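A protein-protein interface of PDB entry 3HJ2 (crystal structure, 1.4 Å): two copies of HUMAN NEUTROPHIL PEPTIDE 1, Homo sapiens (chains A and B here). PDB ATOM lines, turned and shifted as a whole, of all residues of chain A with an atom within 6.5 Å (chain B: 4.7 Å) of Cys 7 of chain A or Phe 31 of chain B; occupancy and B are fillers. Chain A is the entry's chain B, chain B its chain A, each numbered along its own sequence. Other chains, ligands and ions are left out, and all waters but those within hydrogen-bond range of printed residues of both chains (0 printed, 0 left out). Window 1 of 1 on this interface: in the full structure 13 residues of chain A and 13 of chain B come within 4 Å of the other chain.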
ATOM      1  N   CYS A   5      16.261 -13.528  -1.456  1.00  0.00           N
ATOM      2  CA  CYS A   5      15.011 -12.961  -1.954  1.00  0.00           C
ATOM      3  C   CYS A   5      14.322 -12.073  -0.929  1.00  0.00           C
ATOM      4  O   CYS A   5      14.622 -12.114   0.293  1.00  0.00           O
ATOM      5  CB  CYS A   5      14.071 -14.075  -2.363  1.00  0.00           C
ATOM      6  SG  CYS A   5      14.856 -15.247  -3.549  1.00  0.00           S
ATOM      7  N   TYR A   6      13.364 -11.282  -1.404  1.00  0.00           N
ATOM      8  CA  TYR A   6      12.647 -10.349  -0.555  1.00  0.00           C
ATOM      9  C   TYR A   6      11.190 -10.363  -0.869  1.00  0.00           C
ATOM     10  O   TYR A   6      10.759 -10.833  -1.945  1.00  0.00           O
ATOM     11  CB  TYR A   6      13.175  -8.940  -0.798  1.00  0.00           C
ATOM     12  CG  TYR A   6      14.671  -8.798  -0.709  1.00  0.00           C
ATOM     13  CD1 TYR A   6      15.270  -8.521   0.501  1.00  0.00           C
ATOM     14  CD2 TYR A   6      15.469  -8.900  -1.838  1.00  0.00           C
ATOM     15  CE1 TYR A   6      16.657  -8.378   0.599  1.00  0.00           C
ATOM     16  CE2 TYR A   6      16.872  -8.746  -1.754  1.00  0.00           C
ATOM     17  CZ  TYR A   6      17.445  -8.491  -0.534  1.00  0.00           C
ATOM     18  OH  TYR A   6      18.816  -8.337  -0.412  1.00  0.00           O
ATOM     19  N   CYS A   7      10.417  -9.812   0.067  1.00  0.00           N
ATOM     20  CA  CYS A   7       8.990  -9.546  -0.142  1.00  0.00           C
ATOM     21  C   CYS A   7       8.805  -8.028  -0.226  1.00  0.00           C
ATOM     22  O   CYS A   7       9.240  -7.283   0.664  1.00  0.00           O
ATOM     23  CB  CYS A   7       8.175 -10.038   1.067  1.00  0.00           C
ATOM     24  SG  CYS A   7       8.349 -11.802   1.255  1.00  0.00           S
ATOM     25  N   ARG A   8       8.190  -7.592  -1.306  1.00  0.00           N
ATOM     26  CA  ARG A   8       8.049  -6.157  -1.584  1.00  0.00           C
ATOM     27  C   ARG A   8       6.636  -5.806  -1.979  1.00  0.00           C
ATOM     28  O   ARG A   8       5.957  -6.586  -2.630  1.00  0.00           O
ATOM     29  CB  ARG A   8       9.034  -5.716  -2.704  1.00  0.00           C
ATOM     30  CG  ARG A   8      10.465  -6.049  -2.450  1.00  0.00           C
ATOM     31  CD  ARG A   8      11.274  -5.249  -3.392  1.00  0.00           C
ATOM     32  NE  ARG A   8      12.677  -5.708  -3.411  1.00  0.00           N
ATOM     33  CZ  ARG A   8      13.593  -5.373  -2.519  1.00  0.00           C
ATOM     34  NH1 ARG A   8      13.257  -4.585  -1.493  1.00  0.00           N
ATOM     35  NH2 ARG A   8      14.843  -5.816  -2.663  1.00  0.00           N
ATOM     36  N   ILE A   9       6.226  -4.592  -1.566  1.00  0.00           N
ATOM     37  CA  ILE A   9       4.988  -3.972  -2.001  1.00  0.00           C
ATOM     38  C   ILE A   9       5.385  -2.601  -2.648  1.00  0.00           C
ATOM     39  O   ILE A   9       6.040  -1.789  -2.008  1.00  0.00           O
ATOM     40  CB  ILE A   9       4.022  -3.783  -0.803  1.00  0.00           C
ATOM     41  CG1 ILE A   9       3.460  -5.175  -0.369  1.00  0.00           C
ATOM     42  CG2 ILE A   9       2.948  -2.771  -1.173  1.00  0.00           C
ATOM     43  CD1 ILE A   9       2.747  -5.105   1.020  1.00  0.00           C
ATOM     44  N   THR A  21       4.618 -15.079  -4.555  1.00  0.00           N
ATOM     45  CA  THR A  21       3.933 -14.189  -3.606  1.00  0.00           C
ATOM     46  C   THR A  21       4.294 -14.580  -2.200  1.00  0.00           C
ATOM     47  O   THR A  21       4.368 -15.748  -1.871  1.00  0.00           O
ATOM     48  CB  THR A  21       2.417 -14.270  -3.840  1.00  0.00           C
ATOM     49  OG1 THR A  21       2.183 -13.879  -5.193  1.00  0.00           O
ATOM     50  CG2 THR A  21       1.591 -13.358  -2.884  1.00  0.00           C
ATOM     51  N   CYS A  22       4.438 -13.583  -1.336  1.00  0.00           N
ATOM     52  CA  CYS A  22       4.624 -13.859   0.088  1.00  0.00           C
ATOM     53  C   CYS A  22       3.336 -13.524   0.798  1.00  0.00           C
ATOM     54  O   CYS A  22       2.673 -12.523   0.471  1.00  0.00           O
ATOM     55  CB  CYS A  22       5.626 -12.901   0.710  1.00  0.00           C
ATOM     56  SG  CYS A  22       7.126 -12.646  -0.160  1.00  0.00           S
ATOM     57  N   ILE A  23       3.048 -14.320   1.804  1.00  0.00           N
ATOM     58  CA  ILE A  23       2.067 -14.017   2.789  1.00  0.00           C
ATOM     59  C   ILE A  23       2.823 -13.672   4.075  1.00  0.00           C
ATOM     60  O   ILE A  23       3.475 -14.531   4.656  1.00  0.00           O
ATOM     61  CB  ILE A  23       1.120 -15.215   3.013  1.00  0.00           C
ATOM     62  CG1 ILE A  23       0.491 -15.632   1.688  1.00  0.00           C
ATOM     63  CG2 ILE A  23       0.091 -14.821   4.061  1.00  0.00           C
ATOM     64  CD1 ILE A  23      -0.194 -16.977   1.740  1.00  0.00           C
ATOM     65  N   TYR A  24       2.766 -12.396   4.444  1.00  0.00           N
ATOM     66  CA  TYR A  24       3.545 -11.921   5.594  1.00  0.00           C
ATOM     67  C   TYR A  24       2.737 -10.884   6.368  1.00  0.00           C
ATOM     68  O   TYR A  24       2.330  -9.889   5.797  1.00  0.00           O
ATOM     69  CB  TYR A  24       4.910 -11.341   5.112  1.00  0.00           C
ATOM     70  CG  TYR A  24       5.722 -10.682   6.233  1.00  0.00           C
ATOM     71  CD1 TYR A  24       6.258 -11.429   7.260  1.00  0.00           C
ATOM     72  CD2 TYR A  24       5.861  -9.295   6.281  1.00  0.00           C
ATOM     73  CE1 TYR A  24       6.946 -10.861   8.294  1.00  0.00           C
ATOM     74  CE2 TYR A  24       6.569  -8.691   7.338  1.00  0.00           C
ATOM     75  CZ  TYR A  24       7.119  -9.491   8.332  1.00  0.00           C
ATOM     76  OH  TYR A  24       7.839  -8.960   9.395  1.00  0.00           O
ATOM     77  N   TRP A  29       2.535  -9.851  -0.728  1.00  0.00           N
ATOM     78  CA  TRP A  29       3.715  -9.150  -1.216  1.00  0.00           C
ATOM     79  C   TRP A  29       4.239  -9.889  -2.439  1.00  0.00           C
ATOM     80  O   TRP A  29       4.046 -11.103  -2.594  1.00  0.00           O
ATOM     81  CB  TRP A  29       4.842  -9.153  -0.170  1.00  0.00           C
ATOM     82  CG  TRP A  29       4.461  -8.763   1.205  1.00  0.00           C
ATOM     83  CD1 TRP A  29       3.588  -9.392   2.026  1.00  0.00           C
ATOM     84  CD2 TRP A  29       4.982  -7.632   1.963  1.00  0.00           C
ATOM     85  NE1 TRP A  29       3.486  -8.728   3.230  1.00  0.00           N
ATOM     86  CE2 TRP A  29       4.344  -7.646   3.218  1.00  0.00           C
ATOM     87  CE3 TRP A  29       5.933  -6.627   1.701  1.00  0.00           C
ATOM     88  CZ2 TRP A  29       4.627  -6.684   4.231  1.00  0.00           C
ATOM     89  CZ3 TRP A  29       6.170  -5.628   2.698  1.00  0.00           C
ATOM     90  CH2 TRP A  29       5.532  -5.680   3.939  1.00  0.00           C
ATOM     91  N   ALA A  30       4.971  -9.172  -3.292  1.00  0.00           N
ATOM     92  CA  ALA A  30       5.719  -9.785  -4.361  1.00  0.00           C
ATOM     93  C   ALA A  30       6.949 -10.487  -3.797  1.00  0.00           C
ATOM     94  O   ALA A  30       7.658  -9.897  -2.989  1.00  0.00           O
ATOM     95  CB  ALA A  30       6.143  -8.696  -5.329  1.00  0.00           C
ATOM     96  N   PHE A  31       7.180 -11.752  -4.182  1.00  0.00           N
ATOM     97  CA  PHE A  31       8.381 -12.517  -3.753  1.00  0.00           C
ATOM     98  C   PHE A  31       9.389 -12.326  -4.908  1.00  0.00           C
ATOM     99  O   PHE A  31       9.131 -12.740  -6.042  1.00  0.00           O
ATOM    100  CB  PHE A  31       8.048 -13.998  -3.555  1.00  0.00           C
ATOM    101  CG  PHE A  31       9.228 -14.800  -3.143  1.00  0.00           C
ATOM    102  CD1 PHE A  31       9.719 -14.679  -1.848  1.00  0.00           C
ATOM    103  CD2 PHE A  31       9.840 -15.691  -4.013  1.00  0.00           C
ATOM    104  CE1 PHE A  31      10.812 -15.438  -1.440  1.00  0.00           C
ATOM    105  CE2 PHE A  31      10.913 -16.462  -3.591  1.00  0.00           C
ATOM    106  CZ  PHE A  31      11.402 -16.321  -2.315  1.00  0.00           C
ATOM    107  N   CYS A  32      10.493 -11.645  -4.599  1.00  0.00           N
ATOM    108  CA  CYS A  32      11.463 -11.111  -5.570  1.00  0.00           C
ATOM    109  C   CYS A  32      12.846 -11.625  -5.302  1.00  0.00           C
ATOM    110  O   CYS A  32      13.293 -11.600  -4.165  1.00  0.00           O
ATOM    111  CB  CYS A  32      11.504  -9.585  -5.388  1.00  0.00           C
ATOM    112  SG  CYS A  32       9.884  -8.780  -5.659  1.00  0.00           S
ATOM    113  N   CYS B   5      15.827 -13.653   2.385  1.00  0.00           N
ATOM    114  CA  CYS B   5      14.933 -14.759   2.798  1.00  0.00           C
ATOM    115  C   CYS B   5      14.851 -15.813   1.697  1.00  0.00           C
ATOM    116  O   CYS B   5      15.331 -15.632   0.575  1.00  0.00           O
ATOM    117  CB  CYS B   5      13.536 -14.188   3.041  1.00  0.00           C
ATOM    118  SG  CYS B   5      13.587 -12.880   4.300  1.00  0.00           S
ATOM    119  N   TYR B   6      14.187 -16.906   2.023  1.00  0.00           N
ATOM    120  CA  TYR B   6      14.018 -18.008   1.087  1.00  0.00           C
ATOM    121  C   TYR B   6      12.705 -18.716   1.393  1.00  0.00           C
ATOM    122  O   TYR B   6      12.082 -18.451   2.446  1.00  0.00           O
ATOM    123  CB  TYR B   6      15.175 -18.992   1.248  1.00  0.00           C
ATOM    124  N   CYS B  12      11.932 -24.197   7.884  1.00  0.00           N
ATOM    125  CA  CYS B  12      13.175 -23.451   7.727  1.00  0.00           C
ATOM    126  C   CYS B  12      14.420 -24.218   8.161  1.00  0.00           C
ATOM    127  O   CYS B  12      14.322 -25.219   8.851  1.00  0.00           O
ATOM    128  CB  CYS B  12      13.035 -22.138   8.523  1.00  0.00           C
ATOM    129  SG  CYS B  12      11.612 -21.127   7.987  1.00  0.00           S
ATOM    130  N   ARG B  17      14.295 -18.481  10.982  1.00  0.00           N
ATOM    131  CA  ARG B  17      12.953 -18.458  11.573  1.00  0.00           C
ATOM    132  C   ARG B  17      11.915 -18.294  10.475  1.00  0.00           C
ATOM    133  O   ARG B  17      12.166 -17.661   9.405  1.00  0.00           O
ATOM    134  CB  ARG B  17      12.816 -17.291  12.575  1.00  0.00           C
ATOM    135  CG  ARG B  17      13.632 -17.508  13.907  1.00  0.00           C
ATOM    136  CD  ARG B  17      13.092 -18.634  14.839  1.00  0.00           C
ATOM    137  NE  ARG B  17      11.696 -18.372  15.147  1.00  0.00           N
ATOM    138  CZ  ARG B  17      11.260 -17.468  16.033  1.00  0.00           C
ATOM    139  NH1 ARG B  17      12.129 -16.819  16.810  1.00  0.00           N
ATOM    140  NH2 ARG B  17       9.946 -17.285  16.188  1.00  0.00           N
ATOM    141  N   ARG B  18      10.734 -18.852  10.750  1.00  0.00           N
ATOM    142  CA  ARG B  18       9.649 -18.748   9.801  1.00  0.00           C
ATOM    143  C   ARG B  18       8.903 -17.450  10.028  1.00  0.00           C
ATOM    144  O   ARG B  18       8.341 -17.235  11.090  1.00  0.00           O
ATOM    145  CB  ARG B  18       8.704 -19.955   9.896  1.00  0.00           C
ATOM    146  CG  ARG B  18       7.635 -19.906   8.864  1.00  0.00           C
ATOM    147  CD  ARG B  18       6.730 -21.142   8.843  1.00  0.00           C
ATOM    148  NE  ARG B  18       5.755 -20.994   7.759  1.00  0.00           N
ATOM    149  CZ  ARG B  18       5.022 -21.979   7.248  1.00  0.00           C
ATOM    150  NH1 ARG B  18       5.152 -23.195   7.709  1.00  0.00           N
ATOM    151  NH2 ARG B  18       4.168 -21.734   6.289  1.00  0.00           N
ATOM    152  N   TYR B  19       8.899 -16.599   8.995  1.00  0.00           N
ATOM    153  CA  TYR B  19       8.231 -15.312   9.075  1.00  0.00           C
ATOM    154  C   TYR B  19       6.885 -15.287   8.392  1.00  0.00           C
ATOM    155  O   TYR B  19       6.106 -14.388   8.635  1.00  0.00           O
ATOM    156  CB  TYR B  19       9.117 -14.220   8.502  1.00  0.00           C
ATOM    157  CG  TYR B  19      10.234 -13.800   9.422  1.00  0.00           C
ATOM    158  CD1 TYR B  19      10.159 -12.610  10.151  1.00  0.00           C
ATOM    159  CD2 TYR B  19      11.409 -14.514   9.466  1.00  0.00           C
ATOM    160  CE1 TYR B  19      11.188 -12.196  11.003  1.00  0.00           C
ATOM    161  CE2 TYR B  19      12.439 -14.167  10.337  1.00  0.00           C
ATOM    162  CZ  TYR B  19      12.345 -12.982  11.069  1.00  0.00           C
ATOM    163  OH  TYR B  19      13.379 -12.664  11.919  1.00  0.00           O
ATOM    164  N   GLY B  20       6.573 -16.295   7.568  1.00  0.00           N
ATOM    165  CA  GLY B  20       5.255 -16.312   6.872  1.00  0.00           C
ATOM    166  C   GLY B  20       5.272 -17.467   5.901  1.00  0.00           C
ATOM    167  O   GLY B  20       5.907 -18.484   6.171  1.00  0.00           O
ATOM    168  N   THR B  21       4.630 -17.262   4.758  1.00  0.00           N
ATOM    169  CA  THR B  21       4.420 -18.348   3.785  1.00  0.00           C
ATOM    170  C   THR B  21       4.730 -17.813   2.399  1.00  0.00           C
ATOM    171  O   THR B  21       4.370 -16.694   2.077  1.00  0.00           O
ATOM    172  CB  THR B  21       2.958 -18.851   3.875  1.00  0.00           C
ATOM    173  OG1 THR B  21       2.778 -19.363   5.207  1.00  0.00           O
ATOM    174  CG2 THR B  21       2.648 -19.965   2.887  1.00  0.00           C
ATOM    175  N   CYS B  22       5.320 -18.655   1.555  1.00  0.00           N
ATOM    176  CA  CYS B  22       5.405 -18.315   0.138  1.00  0.00           C
ATOM    177  C   CYS B  22       4.393 -19.073  -0.694  1.00  0.00           C
ATOM    178  O   CYS B  22       4.113 -20.235  -0.421  1.00  0.00           O
ATOM    179  CB  CYS B  22       6.741 -18.755  -0.488  1.00  0.00           C
ATOM    180  SG  CYS B  22       8.160 -18.369   0.534  1.00  0.00           S
ATOM    181  N   TRP B  29       4.990 -22.762   0.735  1.00  0.00           N
ATOM    182  CA  TRP B  29       6.298 -22.968   1.322  1.00  0.00           C
ATOM    183  C   TRP B  29       6.438 -22.132   2.588  1.00  0.00           C
ATOM    184  O   TRP B  29       5.802 -21.093   2.719  1.00  0.00           O
ATOM    185  CB  TRP B  29       7.433 -22.484   0.353  1.00  0.00           C
ATOM    186  CG  TRP B  29       7.294 -22.978  -1.040  1.00  0.00           C
ATOM    187  CD1 TRP B  29       6.258 -22.716  -1.909  1.00  0.00           C
ATOM    188  CD2 TRP B  29       8.210 -23.850  -1.753  1.00  0.00           C
ATOM    189  NE1 TRP B  29       6.478 -23.368  -3.106  1.00  0.00           N
ATOM    190  CE2 TRP B  29       7.663 -24.073  -3.034  1.00  0.00           C
ATOM    191  CE3 TRP B  29       9.438 -24.460  -1.430  1.00  0.00           C
ATOM    192  CZ2 TRP B  29       8.304 -24.876  -3.990  1.00  0.00           C
ATOM    193  CZ3 TRP B  29      10.050 -25.276  -2.373  1.00  0.00           C
ATOM    194  CH2 TRP B  29       9.476 -25.471  -3.632  1.00  0.00           C
ATOM    195  N   ALA B  30       7.351 -22.576   3.461  1.00  0.00           N
ATOM    196  CA  ALA B  30       7.722 -21.719   4.568  1.00  0.00           C
ATOM    197  C   ALA B  30       8.574 -20.552   4.048  1.00  0.00           C
ATOM    198  O   ALA B  30       9.482 -20.758   3.300  1.00  0.00           O
ATOM    199  CB  ALA B  30       8.522 -22.542   5.596  1.00  0.00           C
ATOM    200  N   PHE B  31       8.268 -19.312   4.469  1.00  0.00           N
ATOM    201  CA  PHE B  31       9.079 -18.134   4.193  1.00  0.00           C
ATOM    202  C   PHE B  31      10.009 -17.939   5.398  1.00  0.00           C
ATOM    203  O   PHE B  31       9.537 -17.715   6.527  1.00  0.00           O
ATOM    204  CB  PHE B  31       8.156 -16.943   3.987  1.00  0.00           C
ATOM    205  CG  PHE B  31       8.853 -15.614   3.812  1.00  0.00           C
ATOM    206  CD1 PHE B  31       9.696 -15.383   2.722  1.00  0.00           C
ATOM    207  CD2 PHE B  31       8.677 -14.584   4.765  1.00  0.00           C
ATOM    208  CE1 PHE B  31      10.293 -14.153   2.553  1.00  0.00           C
ATOM    209  CE2 PHE B  31       9.304 -13.363   4.624  1.00  0.00           C
ATOM    210  CZ  PHE B  31      10.142 -13.170   3.542  1.00  0.00           C
ATOM    211  N   CYS B  32      11.305 -18.015   5.097  1.00  0.00           N
ATOM    212  CA  CYS B  32      12.325 -18.178   6.118  1.00  0.00           C
ATOM    213  C   CYS B  32      13.348 -17.064   6.023  1.00  0.00           C
ATOM    214  O   CYS B  32      13.802 -16.800   4.900  1.00  0.00           O
ATOM    215  CB  CYS B  32      13.038 -19.476   5.854  1.00  0.00           C
ATOM    216  SG  CYS B  32      11.936 -20.914   5.987  1.00  0.00           S
ATOM    217  N   CYS B  33      13.756 -16.466   7.148  1.00  0.00           N
ATOM    218  CA  CYS B  33      14.806 -15.427   7.142  1.00  0.00           C
ATOM    219  C   CYS B  33      15.748 -15.644   8.321  1.00  0.00           C
ATOM    220  O   CYS B  33      16.868 -15.079   8.306  1.00  0.00           O
ATOM    221  CB  CYS B  33      14.204 -14.003   7.176  1.00  0.00           C
ATOM    222  SG  CYS B  33      12.828 -13.725   6.047  1.00  0.00           S
ATOM    223  OXT CYS B  33      15.361 -16.342   9.288  1.00  0.00           O
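O of Cys 5 of chain A is in hydrogen-bond range of N of Cys 5 of chain B, at 2.9 Å.
The backbone carbonyl oxygen of Thr 21 of chain B sits at hydrogen-bond distance from the backbone NH of Ile 23 of chain A (2.7 Å).
The side-chain sulfur (SG) of Cys 5 of chain B is disulfide-bonded to the side-chain sulfur (SG) of Cys 33 of chain B (2.1 Å).
O of Gly 20 of chain B is in hydrogen-bond range of NE of Arg 18 of chain B (3.0 Å).
The guanidinium group (NH2) of Arg 18 of chain B sits at hydrogen-bond distance from the side-chain hydroxyl (OG1) of Thr 21 of chain B.
The backbone carbonyl oxygen (O) of Gly 20 of chain B lies within hydrogen-bond range of the backbone NH (N) of Phe 31 of chain B (3.0 Å).
SG of Cys 7 of chain A forms a disulfide with SG of Cys 22 of chain A, at 2.1 Å.
The backbone NH (N) of Cys 22 of chain A is in hydrogen-bond range of the backbone carbonyl oxygen (O) of Trp 29 of chain A, at 2.8 Å.
Among the printed residues, pairs that only touch across the chains: Cys 7 of chain A with Phe 31 of chain B (3.2 Å), Tyr 24 of chain A with Tyr 19 of chain B (3.3 Å), Ile 23 of chain A with Gly 20 of chain B (3.4 Å), Thr 21 of chain A with Cys 22 of chain B (3.4 Å) and Cys 22 of chain A with Thr 21 of chain B (3.5 Å).
Printed residues of chain B within 4 Å of Cys 5 of chain A: Cys 5.
Cys 7 of chain A touches just one residue of chain B: Phe 31.
Of the printed residues of chain A, Cys 5 of chain B touches Cys 5 (2.9 Å).
Arg 18 of chain B touches none of the printed residues of chain A.
Printed residues of chain A within 4 Å of Gly 20 of chain B: Ile 23.
Of the printed residues of chain A, Cys 22 of chain B touches Thr 21.
The nearest residue of chain A that does not touch Phe 31 of chain B is Phe 31 of chain A (4.2 Å).
The nearest printed residue of chain A that does not touch Thr 21 of chain B is Thr 21 of chain A (4.1 Å).
Of the 13 printed residues of chain A, 6 touch a printed residue of chain B.
Along chain A the printed residues that touch a printed residue of chain B span positions 5 to 24.
Among the printed residues, 7 pairs touch across the chains.
Among the printed residues, no Asp or Glu carboxylate lies within 4 Å of a Lys or Arg side-chain nitrogen of the other chain.
Cys 5 of chain A touches its own counterpart, Cys 5 of chain B.
Thr 21 of chain A touches Cys 22 of chain B, and with the chains exchanged Cys 22 of chain A touches Thr 21 of chain B.
Of the 7 pairs that touch across the chains among the printed residues, 3 have their exchanged pair printed and touching as well.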
